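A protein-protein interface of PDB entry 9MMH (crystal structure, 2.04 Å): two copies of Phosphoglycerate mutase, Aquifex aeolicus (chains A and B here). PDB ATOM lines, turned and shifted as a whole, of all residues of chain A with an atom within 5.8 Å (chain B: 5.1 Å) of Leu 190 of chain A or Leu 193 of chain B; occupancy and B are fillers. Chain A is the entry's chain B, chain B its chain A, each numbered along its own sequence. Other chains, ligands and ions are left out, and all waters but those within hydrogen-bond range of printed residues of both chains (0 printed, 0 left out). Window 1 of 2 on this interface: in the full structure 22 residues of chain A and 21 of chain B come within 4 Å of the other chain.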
ATOM      1  N   LEU A 157      13.042   3.767  -7.476  1.00  0.00           N
ATOM      2  CA  LEU A 157      12.870   4.726  -6.382  1.00  0.00           C
ATOM      3  C   LEU A 157      12.309   6.045  -6.886  1.00  0.00           C
ATOM      4  O   LEU A 157      11.388   6.614  -6.293  1.00  0.00           O
ATOM      5  CB  LEU A 157      14.211   4.981  -5.674  1.00  0.00           C
ATOM      6  CG  LEU A 157      14.669   3.985  -4.641  1.00  0.00           C
ATOM      7  CD1 LEU A 157      15.880   4.549  -3.856  1.00  0.00           C
ATOM      8  CD2 LEU A 157      13.534   3.650  -3.697  1.00  0.00           C
ATOM      9  N   LEU A 161       8.575   7.472  -5.605  1.00  0.00           N
ATOM     10  CA  LEU A 161       8.450   8.737  -4.895  1.00  0.00           C
ATOM     11  C   LEU A 161       7.894   9.854  -5.758  1.00  0.00           C
ATOM     12  O   LEU A 161       7.654  10.954  -5.241  1.00  0.00           O
ATOM     13  CB  LEU A 161       9.822   9.157  -4.356  1.00  0.00           C
ATOM     14  CG  LEU A 161      10.457   8.094  -3.439  1.00  0.00           C
ATOM     15  CD1 LEU A 161      11.774   8.655  -2.865  1.00  0.00           C
ATOM     16  CD2 LEU A 161       9.506   7.648  -2.328  1.00  0.00           C
ATOM     17  N   SER A 179      18.060  -0.636   0.210  1.00  0.00           N
ATOM     18  CA  SER A 179      17.193   0.521   0.375  1.00  0.00           C
ATOM     19  C   SER A 179      15.775   0.026   0.569  1.00  0.00           C
ATOM     20  O   SER A 179      15.229  -0.679  -0.295  1.00  0.00           O
ATOM     21  CB  SER A 179      17.267   1.473  -0.818  1.00  0.00           C
ATOM     22  OG  SER A 179      18.617   1.669  -1.166  1.00  0.00           O
ATOM     23  N   LEU A 180      15.190   0.375   1.710  1.00  0.00           N
ATOM     24  CA  LEU A 180      13.870  -0.093   2.090  1.00  0.00           C
ATOM     25  C   LEU A 180      12.817   0.908   1.650  1.00  0.00           C
ATOM     26  O   LEU A 180      12.839   2.086   2.046  1.00  0.00           O
ATOM     27  CB  LEU A 180      13.817  -0.354   3.597  1.00  0.00           C
ATOM     28  CG  LEU A 180      12.394  -0.574   4.102  1.00  0.00           C
ATOM     29  CD1 LEU A 180      11.721  -1.819   3.438  1.00  0.00           C
ATOM     30  CD2 LEU A 180      12.424  -0.763   5.628  1.00  0.00           C
ATOM     31  N   LEU A 181      11.900   0.429   0.821  1.00  0.00           N
ATOM     32  CA  LEU A 181      10.768   1.175   0.313  1.00  0.00           C
ATOM     33  C   LEU A 181       9.503   0.554   0.874  1.00  0.00           C
ATOM     34  O   LEU A 181       9.309  -0.659   0.764  1.00  0.00           O
ATOM     35  CB  LEU A 181      10.742   1.114  -1.208  1.00  0.00           C
ATOM     36  CG  LEU A 181       9.936   2.116  -2.002  1.00  0.00           C
ATOM     37  CD1 LEU A 181      10.471   3.521  -1.896  1.00  0.00           C
ATOM     38  CD2 LEU A 181       9.966   1.604  -3.476  1.00  0.00           C
ATOM     39  N   GLU A 182       8.681   1.355   1.534  1.00  0.00           N
ATOM     40  CA  GLU A 182       7.427   0.857   2.081  1.00  0.00           C
ATOM     41  C   GLU A 182       6.260   1.429   1.293  1.00  0.00           C
ATOM     42  O   GLU A 182       6.319   2.553   0.776  1.00  0.00           O
ATOM     43  CB  GLU A 182       7.271   1.190   3.564  1.00  0.00           C
ATOM     44  CG  GLU A 182       8.230   0.420   4.462  1.00  0.00           C
ATOM     45  CD  GLU A 182       7.975   0.625   5.949  1.00  0.00           C
ATOM     46  OE1 GLU A 182       7.218   1.540   6.301  1.00  0.00           O
ATOM     47  OE2 GLU A 182       8.510  -0.136   6.757  1.00  0.00           O
ATOM     48  N   PHE A 188       4.156   5.525  -1.456  1.00  0.00           N
ATOM     49  CA  PHE A 188       5.421   4.942  -1.058  1.00  0.00           C
ATOM     50  C   PHE A 188       6.126   5.840  -0.047  1.00  0.00           C
ATOM     51  O   PHE A 188       5.920   7.062  -0.020  1.00  0.00           O
ATOM     52  CB  PHE A 188       6.293   4.763  -2.296  1.00  0.00           C
ATOM     53  CG  PHE A 188       5.874   3.617  -3.204  1.00  0.00           C
ATOM     54  CD1 PHE A 188       6.267   2.318  -2.937  1.00  0.00           C
ATOM     55  CD2 PHE A 188       5.134   3.860  -4.349  1.00  0.00           C
ATOM     56  CE1 PHE A 188       5.911   1.276  -3.789  1.00  0.00           C
ATOM     57  CE2 PHE A 188       4.797   2.814  -5.212  1.00  0.00           C
ATOM     58  CZ  PHE A 188       5.169   1.544  -4.923  1.00  0.00           C
ATOM     59  N   TYR A 189       6.980   5.210   0.769  1.00  0.00           N
ATOM     60  CA  TYR A 189       7.810   5.901   1.748  1.00  0.00           C
ATOM     61  C   TYR A 189       9.203   5.291   1.708  1.00  0.00           C
ATOM     62  O   TYR A 189       9.341   4.080   1.902  1.00  0.00           O
ATOM     63  CB  TYR A 189       7.271   5.783   3.186  1.00  0.00           C
ATOM     64  CG  TYR A 189       5.819   6.120   3.350  1.00  0.00           C
ATOM     65  CD1 TYR A 189       4.833   5.156   3.131  1.00  0.00           C
ATOM     66  CD2 TYR A 189       5.417   7.397   3.740  1.00  0.00           C
ATOM     67  CE1 TYR A 189       3.495   5.455   3.274  1.00  0.00           C
ATOM     68  CE2 TYR A 189       4.064   7.712   3.887  1.00  0.00           C
ATOM     69  CZ  TYR A 189       3.115   6.738   3.647  1.00  0.00           C
ATOM     70  OH  TYR A 189       1.774   7.023   3.797  1.00  0.00           O
ATOM     71  N   LEU A 190      10.234   6.128   1.522  1.00  0.00           N
ATOM     72  CA  LEU A 190      11.617   5.652   1.495  1.00  0.00           C
ATOM     73  C   LEU A 190      12.164   5.685   2.908  1.00  0.00           C
ATOM     74  O   LEU A 190      12.322   6.762   3.501  1.00  0.00           O
ATOM     75  CB  LEU A 190      12.455   6.492   0.553  1.00  0.00           C
ATOM     76  CG  LEU A 190      13.865   5.991   0.353  1.00  0.00           C
ATOM     77  CD1 LEU A 190      13.929   4.646  -0.302  1.00  0.00           C
ATOM     78  CD2 LEU A 190      14.693   6.973  -0.468  1.00  0.00           C
ATOM     79  N   LYS A 191      12.444   4.508   3.456  1.00  0.00           N
ATOM     80  CA  LYS A 191      12.919   4.418   4.815  1.00  0.00           C
ATOM     81  C   LYS A 191      14.429   4.379   4.930  1.00  0.00           C
ATOM     82  O   LYS A 191      14.955   4.669   6.005  1.00  0.00           O
ATOM     83  CB  LYS A 191      12.333   3.201   5.507  1.00  0.00           C
ATOM     84  CG  LYS A 191      10.830   3.100   5.359  1.00  0.00           C
ATOM     85  CD  LYS A 191      10.073   4.098   6.201  1.00  0.00           C
ATOM     86  CE  LYS A 191      10.269   3.835   7.677  1.00  0.00           C
ATOM     87  NZ  LYS A 191       9.645   2.552   8.107  1.00  0.00           N
ATOM     88  N   SER A 192      15.138   4.016   3.873  1.00  0.00           N
ATOM     89  CA  SER A 192      16.593   4.004   3.930  1.00  0.00           C
ATOM     90  C   SER A 192      17.087   3.928   2.498  1.00  0.00           C
ATOM     91  O   SER A 192      16.351   3.515   1.595  1.00  0.00           O
ATOM     92  CB  SER A 192      17.137   2.825   4.731  1.00  0.00           C
ATOM     93  OG  SER A 192      16.790   1.617   4.080  1.00  0.00           O
ATOM     94  N   LEU A 193      18.341   4.335   2.311  1.00  0.00           N
ATOM     95  CA  LEU A 193      19.026   4.243   1.024  1.00  0.00           C
ATOM     96  C   LEU A 193      20.460   3.832   1.275  1.00  0.00           C
ATOM     97  O   LEU A 193      21.176   4.453   2.095  1.00  0.00           O
ATOM     98  CB  LEU A 193      18.982   5.574   0.263  1.00  0.00           C
ATOM     99  CG  LEU A 193      19.811   5.636  -1.021  1.00  0.00           C
ATOM    100  CD1 LEU A 193      19.036   4.958  -2.195  1.00  0.00           C
ATOM    101  CD2 LEU A 193      20.199   7.066  -1.404  1.00  0.00           C
ATOM    102  N   ASN A 194      20.872   2.788   0.548  1.00  0.00           N
ATOM    103  CA  ASN A 194      22.263   2.341   0.466  1.00  0.00           C
ATOM    104  C   ASN A 194      22.831   1.962   1.830  1.00  0.00           C
ATOM    105  O   ASN A 194      23.966   2.314   2.195  1.00  0.00           O
ATOM    106  CB  ASN A 194      23.121   3.390  -0.220  1.00  0.00           C
ATOM    107  CG  ASN A 194      24.466   2.845  -0.601  1.00  0.00           C
ATOM    108  OD1 ASN A 194      24.605   1.642  -0.805  1.00  0.00           O
ATOM    109  ND2 ASN A 194      25.455   3.703  -0.706  1.00  0.00           N
ATOM    110  N   LEU B 157      17.437  17.961   2.462  1.00  0.00           N
ATOM    111  CA  LEU B 157      17.648  16.941   1.424  1.00  0.00           C
ATOM    112  C   LEU B 157      16.829  17.253   0.178  1.00  0.00           C
ATOM    113  O   LEU B 157      17.336  17.198  -0.946  1.00  0.00           O
ATOM    114  CB  LEU B 157      17.261  15.557   1.931  1.00  0.00           C
ATOM    115  CG  LEU B 157      18.340  14.801   2.648  1.00  0.00           C
ATOM    116  CD1 LEU B 157      18.041  13.305   2.686  1.00  0.00           C
ATOM    117  CD2 LEU B 157      19.698  15.063   2.013  1.00  0.00           C
ATOM    118  N   HIS B 170       8.147  12.031   2.307  1.00  0.00           N
ATOM    119  CA  HIS B 170       8.314  10.815   1.530  1.00  0.00           C
ATOM    120  C   HIS B 170       9.581  10.059   1.906  1.00  0.00           C
ATOM    121  O   HIS B 170       9.818   8.971   1.377  1.00  0.00           O
ATOM    122  CB  HIS B 170       8.369  11.165   0.033  1.00  0.00           C
ATOM    123  CG  HIS B 170       7.030  11.407  -0.589  1.00  0.00           C
ATOM    124  ND1 HIS B 170       6.253  12.501  -0.279  1.00  0.00           N
ATOM    125  CD2 HIS B 170       6.323  10.683  -1.492  1.00  0.00           C
ATOM    126  CE1 HIS B 170       5.140  12.463  -0.992  1.00  0.00           C
ATOM    127  NE2 HIS B 170       5.145  11.355  -1.713  1.00  0.00           N
ATOM    128  N   ILE B 171      10.417  10.643   2.751  1.00  0.00           N
ATOM    129  CA  ILE B 171      11.647  10.028   3.213  1.00  0.00           C
ATOM    130  C   ILE B 171      11.568   9.979   4.730  1.00  0.00           C
ATOM    131  O   ILE B 171      10.846  10.754   5.355  1.00  0.00           O
ATOM    132  CB  ILE B 171      12.901  10.786   2.744  1.00  0.00           C
ATOM    133  CG1 ILE B 171      12.856  12.246   3.171  1.00  0.00           C
ATOM    134  CG2 ILE B 171      13.043  10.716   1.243  1.00  0.00           C
ATOM    135  CD1 ILE B 171      14.076  13.000   2.761  1.00  0.00           C
ATOM    136  N   HIS B 172      12.333   9.070   5.319  1.00  0.00           N
ATOM    137  CA  HIS B 172      12.375   8.955   6.764  1.00  0.00           C
ATOM    138  C   HIS B 172      13.803   8.951   7.314  1.00  0.00           C
ATOM    139  O   HIS B 172      14.749   8.496   6.666  1.00  0.00           O
ATOM    140  CB  HIS B 172      11.629   7.701   7.167  1.00  0.00           C
ATOM    141  CG  HIS B 172      11.575   7.499   8.636  1.00  0.00           C
ATOM    142  ND1 HIS B 172      10.980   8.410   9.490  1.00  0.00           N
ATOM    143  CD2 HIS B 172      12.092   6.519   9.411  1.00  0.00           C
ATOM    144  CE1 HIS B 172      11.129   7.985  10.730  1.00  0.00           C
ATOM    145  NE2 HIS B 172      11.798   6.840  10.709  1.00  0.00           N
ATOM    146  N   MET B 173      13.953   9.473   8.550  1.00  0.00           N
ATOM    147  CA  MET B 173      15.175   9.305   9.323  1.00  0.00           C
ATOM    148  C   MET B 173      14.846   8.885  10.749  1.00  0.00           C
ATOM    149  O   MET B 173      14.005   9.506  11.404  1.00  0.00           O
ATOM    150  CB  MET B 173      16.024  10.586   9.316  1.00  0.00           C
ATOM    151  CG  MET B 173      16.103  11.267   7.970  1.00  0.00           C
ATOM    152  SD  MET B 173      17.027  12.843   8.080  1.00  0.00           S
ATOM    153  CE  MET B 173      18.589  12.225   8.108  1.00  0.00           C
ATOM    154  N   ILE B 178      21.877   8.759   9.928  1.00  0.00           N
ATOM    155  CA  ILE B 178      22.847   9.585   9.218  1.00  0.00           C
ATOM    156  C   ILE B 178      22.565   9.494   7.730  1.00  0.00           C
ATOM    157  O   ILE B 178      22.382   8.384   7.192  1.00  0.00           O
ATOM    158  CB  ILE B 178      24.279   9.094   9.497  1.00  0.00           C
ATOM    159  CG1 ILE B 178      24.621   9.127  10.979  1.00  0.00           C
ATOM    160  CG2 ILE B 178      25.274   9.818   8.635  1.00  0.00           C
ATOM    161  CD1 ILE B 178      25.835   8.304  11.300  1.00  0.00           C
ATOM    162  N   SER B 179      22.599  10.632   7.047  1.00  0.00           N
ATOM    163  CA  SER B 179      22.449  10.674   5.597  1.00  0.00           C
ATOM    164  C   SER B 179      23.557  11.523   4.997  1.00  0.00           C
ATOM    165  O   SER B 179      23.679  12.717   5.328  1.00  0.00           O
ATOM    166  CB  SER B 179      21.088  11.236   5.234  1.00  0.00           C
ATOM    167  OG  SER B 179      20.063  10.595   5.935  1.00  0.00           O
ATOM    168  N   LEU B 190      23.073  12.278  -3.190  1.00  0.00           N
ATOM    169  CA  LEU B 190      22.735  11.580  -1.954  1.00  0.00           C
ATOM    170  C   LEU B 190      23.385  10.192  -1.964  1.00  0.00           C
ATOM    171  O   LEU B 190      23.041   9.331  -2.786  1.00  0.00           O
ATOM    172  CB  LEU B 190      21.226  11.506  -1.814  1.00  0.00           C
ATOM    173  CG  LEU B 190      20.741  10.903  -0.503  1.00  0.00           C
ATOM    174  CD1 LEU B 190      21.274  11.707   0.646  1.00  0.00           C
ATOM    175  CD2 LEU B 190      19.228  10.883  -0.426  1.00  0.00           C
ATOM    176  N   LYS B 191      24.332   9.977  -1.052  1.00  0.00           N
ATOM    177  CA  LYS B 191      25.020   8.701  -0.946  1.00  0.00           C
ATOM    178  C   LYS B 191      24.391   7.723   0.033  1.00  0.00           C
ATOM    179  O   LYS B 191      24.680   6.523  -0.027  1.00  0.00           O
ATOM    180  CB  LYS B 191      26.469   8.939  -0.552  1.00  0.00           C
ATOM    181  CG  LYS B 191      27.163   9.964  -1.452  1.00  0.00           C
ATOM    182  CD  LYS B 191      27.628   9.334  -2.761  1.00  0.00           C
ATOM    183  CE  LYS B 191      28.814   8.354  -2.577  1.00  0.00           C
ATOM    184  NZ  LYS B 191      30.180   8.988  -2.525  1.00  0.00           N
ATOM    185  N   SER B 192      23.562   8.188   0.948  1.00  0.00           N
ATOM    186  CA  SER B 192      22.968   7.293   1.926  1.00  0.00           C
ATOM    187  C   SER B 192      21.830   8.065   2.541  1.00  0.00           C
ATOM    188  O   SER B 192      21.846   9.321   2.554  1.00  0.00           O
ATOM    189  CB  SER B 192      23.966   6.848   2.996  1.00  0.00           C
ATOM    190  OG  SER B 192      24.288   7.953   3.855  1.00  0.00           O
ATOM    191  N   LEU B 193      20.842   7.315   3.042  1.00  0.00           N
ATOM    192  CA  LEU B 193      19.749   7.868   3.823  1.00  0.00           C
ATOM    193  C   LEU B 193      19.452   6.962   5.000  1.00  0.00           C
ATOM    194  O   LEU B 193      19.243   5.748   4.836  1.00  0.00           O
ATOM    195  CB  LEU B 193      18.485   8.038   2.988  1.00  0.00           C
ATOM    196  CG  LEU B 193      17.245   8.528   3.707  1.00  0.00           C
ATOM    197  CD1 LEU B 193      17.264  10.067   3.904  1.00  0.00           C
ATOM    198  CD2 LEU B 193      15.959   8.113   3.014  1.00  0.00           C
ATOM    199  N   ASN B 194      19.388   7.577   6.184  1.00  0.00           N
ATOM    200  CA  ASN B 194      18.964   6.897   7.404  1.00  0.00           C
ATOM    201  C   ASN B 194      19.825   5.686   7.706  1.00  0.00           C
ATOM    202  O   ASN B 194      19.317   4.613   8.039  1.00  0.00           O
ATOM    203  CB  ASN B 194      17.480   6.491   7.327  1.00  0.00           C
ATOM    204  CG  ASN B 194      16.925   6.121   8.693  1.00  0.00           C
ATOM    205  OD1 ASN B 194      17.442   6.584   9.713  1.00  0.00           O
ATOM    206  ND2 ASN B 194      15.881   5.319   8.726  1.00  0.00           N
ATOM    207  N   ASP B 195      21.139   5.885   7.710  1.00  0.00           N
ATOM    208  CA  ASP B 195      22.109   4.886   8.153  1.00  0.00           C
ATOM    209  C   ASP B 195      22.161   4.828   9.679  1.00  0.00           C
ATOM    210  O   ASP B 195      22.557   5.806  10.341  1.00  0.00           O
ATOM    211  CB  ASP B 195      23.443   5.268   7.515  1.00  0.00           C
ATOM    212  CG  ASP B 195      24.636   4.475   8.007  1.00  0.00           C
ATOM    213  OD1 ASP B 195      24.555   3.613   8.938  1.00  0.00           O
ATOM    214  OD2 ASP B 195      25.713   4.782   7.433  1.00  0.00           O
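Leu 190 of chain A touches Leu 193 of chain B, and with the chains exchanged Leu 193 of chain A touches Leu 190 of chain B. Lys 191 of chain A touches Asn 194 of chain B, and with the chains exchanged Asn 194 of chain A touches Lys 191 of chain B. Ser 192 of chain A touches Leu 193 of chain B, and with the chains exchanged Leu 193 of chain A touches Ser 192 of chain B. Leu 193 of chain A touches its own counterpart, Leu 193 of chain B. Positions printed for both chains: 157, 179, 190, 191, 192, 193 and 194. Of the 14 pairs that touch across the chains among the printed residues, 7 have their exchanged pair printed and touching as well.
Printed residues of chain B within 4 Å of Tyr 189 of chain A: His 170. Leu 190 of chain A touches just these residues of chain B: His 170 (2.9 Å), Ile 171 (3.3 Å), His 172 (2.9 Å) and Leu 193 (3.9 Å). Printed residues of chain B within 4 Å of Leu 193 of chain A: Leu 190 (3.9 Å), Ser 192 (3.4 Å) and Leu 193 (3.0 Å). Of the printed residues of chain A, His 170 of chain B touches Leu 161, Phe 188, Tyr 189 and Leu 190. Of the printed residues of chain A, Ile 171 of chain B touches Leu 190. Of the printed residues of chain A, Ser 192 of chain B touches Leu 193 (3.4 Å). The nearest printed residue of chain B that does not touch Leu 190 of chain A is Met 173 of chain B (6.0 Å). The nearest residue of chain A that does not touch Leu 193 of chain B is Lys 191 of chain A (4.5 Å).
O of Lys 191 of chain A sits at hydrogen-bond distance from ND2 of Asn 194 of chain B (2.9 Å). The backbone NH (N) of Leu 193 of chain A is in hydrogen-bond range of the backbone carbonyl oxygen (O) of Leu 193 of chain B, at 3.0 Å. The backbone NH (N) of His 172 of chain B sits at hydrogen-bond distance from the backbone carbonyl oxygen (O) of Leu 190 of chain A, 2.9 Å away. The side-chain amide nitrogen of Asn 194 of chain A sits at hydrogen-bond distance from the backbone carbonyl oxygen of Lys 191 of chain B (3.0 Å). O of His 170 of chain B sits at hydrogen-bond distance from N of Leu 190 of chain A (2.9 Å).
Among the printed residues, merely in contact across the chains: Ser 192 of chain A with Leu 193 of chain B, Leu 190 of chain A with Ile 171 of chain B, Leu 193 of chain A with Ser 192 of chain B, Lys 191 of chain A with His 172 of chain B, Tyr 189 of chain A with His 170 of chain B, Leu 190 of chain A with Leu 193 of chain B, Leu 193 of chain A with Leu 190 of chain B, Phe 188 of chain A with His 170 of chain B and Leu 161 of chain A with His 170 of chain B.
Hydrophobic or aromatic side chains of chain B within 4 Å of the printed part of chain A: His 170, His 172, Leu 190 and Leu 193. Along chain A the printed residues that touch a printed residue of chain B span positions 161 to 194. Among the printed residues, no Asp or Glu carboxylate lies within 4 Å of a Lys or Arg side-chain nitrogen of the other chain.
The side-chain hydroxyl (OG) of Ser 179 of chain A sits at hydrogen-bond distance from the backbone NH (N) of Asn 194 of chain A, 3.0 Å away. The side-chain hydroxyl of Ser 179 of chain B lies within hydrogen-bond range of the backbone NH of Asn 194 of chain B, at 3.1 Å. The backbone NH (N) of Tyr 189 of chain A is in hydrogen-bond range of the backbone carbonyl oxygen (O) of Glu 182 of chain A. N of Leu 180 of chain A lies within hydrogen-bond range of OG of Ser 192 of chain A, 3.1 Å away. The backbone NH of Asn 194 of chain B is in hydrogen-bond range of the backbone carbonyl oxygen of Ile 178 of chain B (3.3 Å). The backbone carbonyl oxygen (O) of Leu 180 of chain A lies within hydrogen-bond range of the backbone NH (N) of Lys 191 of chain A.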
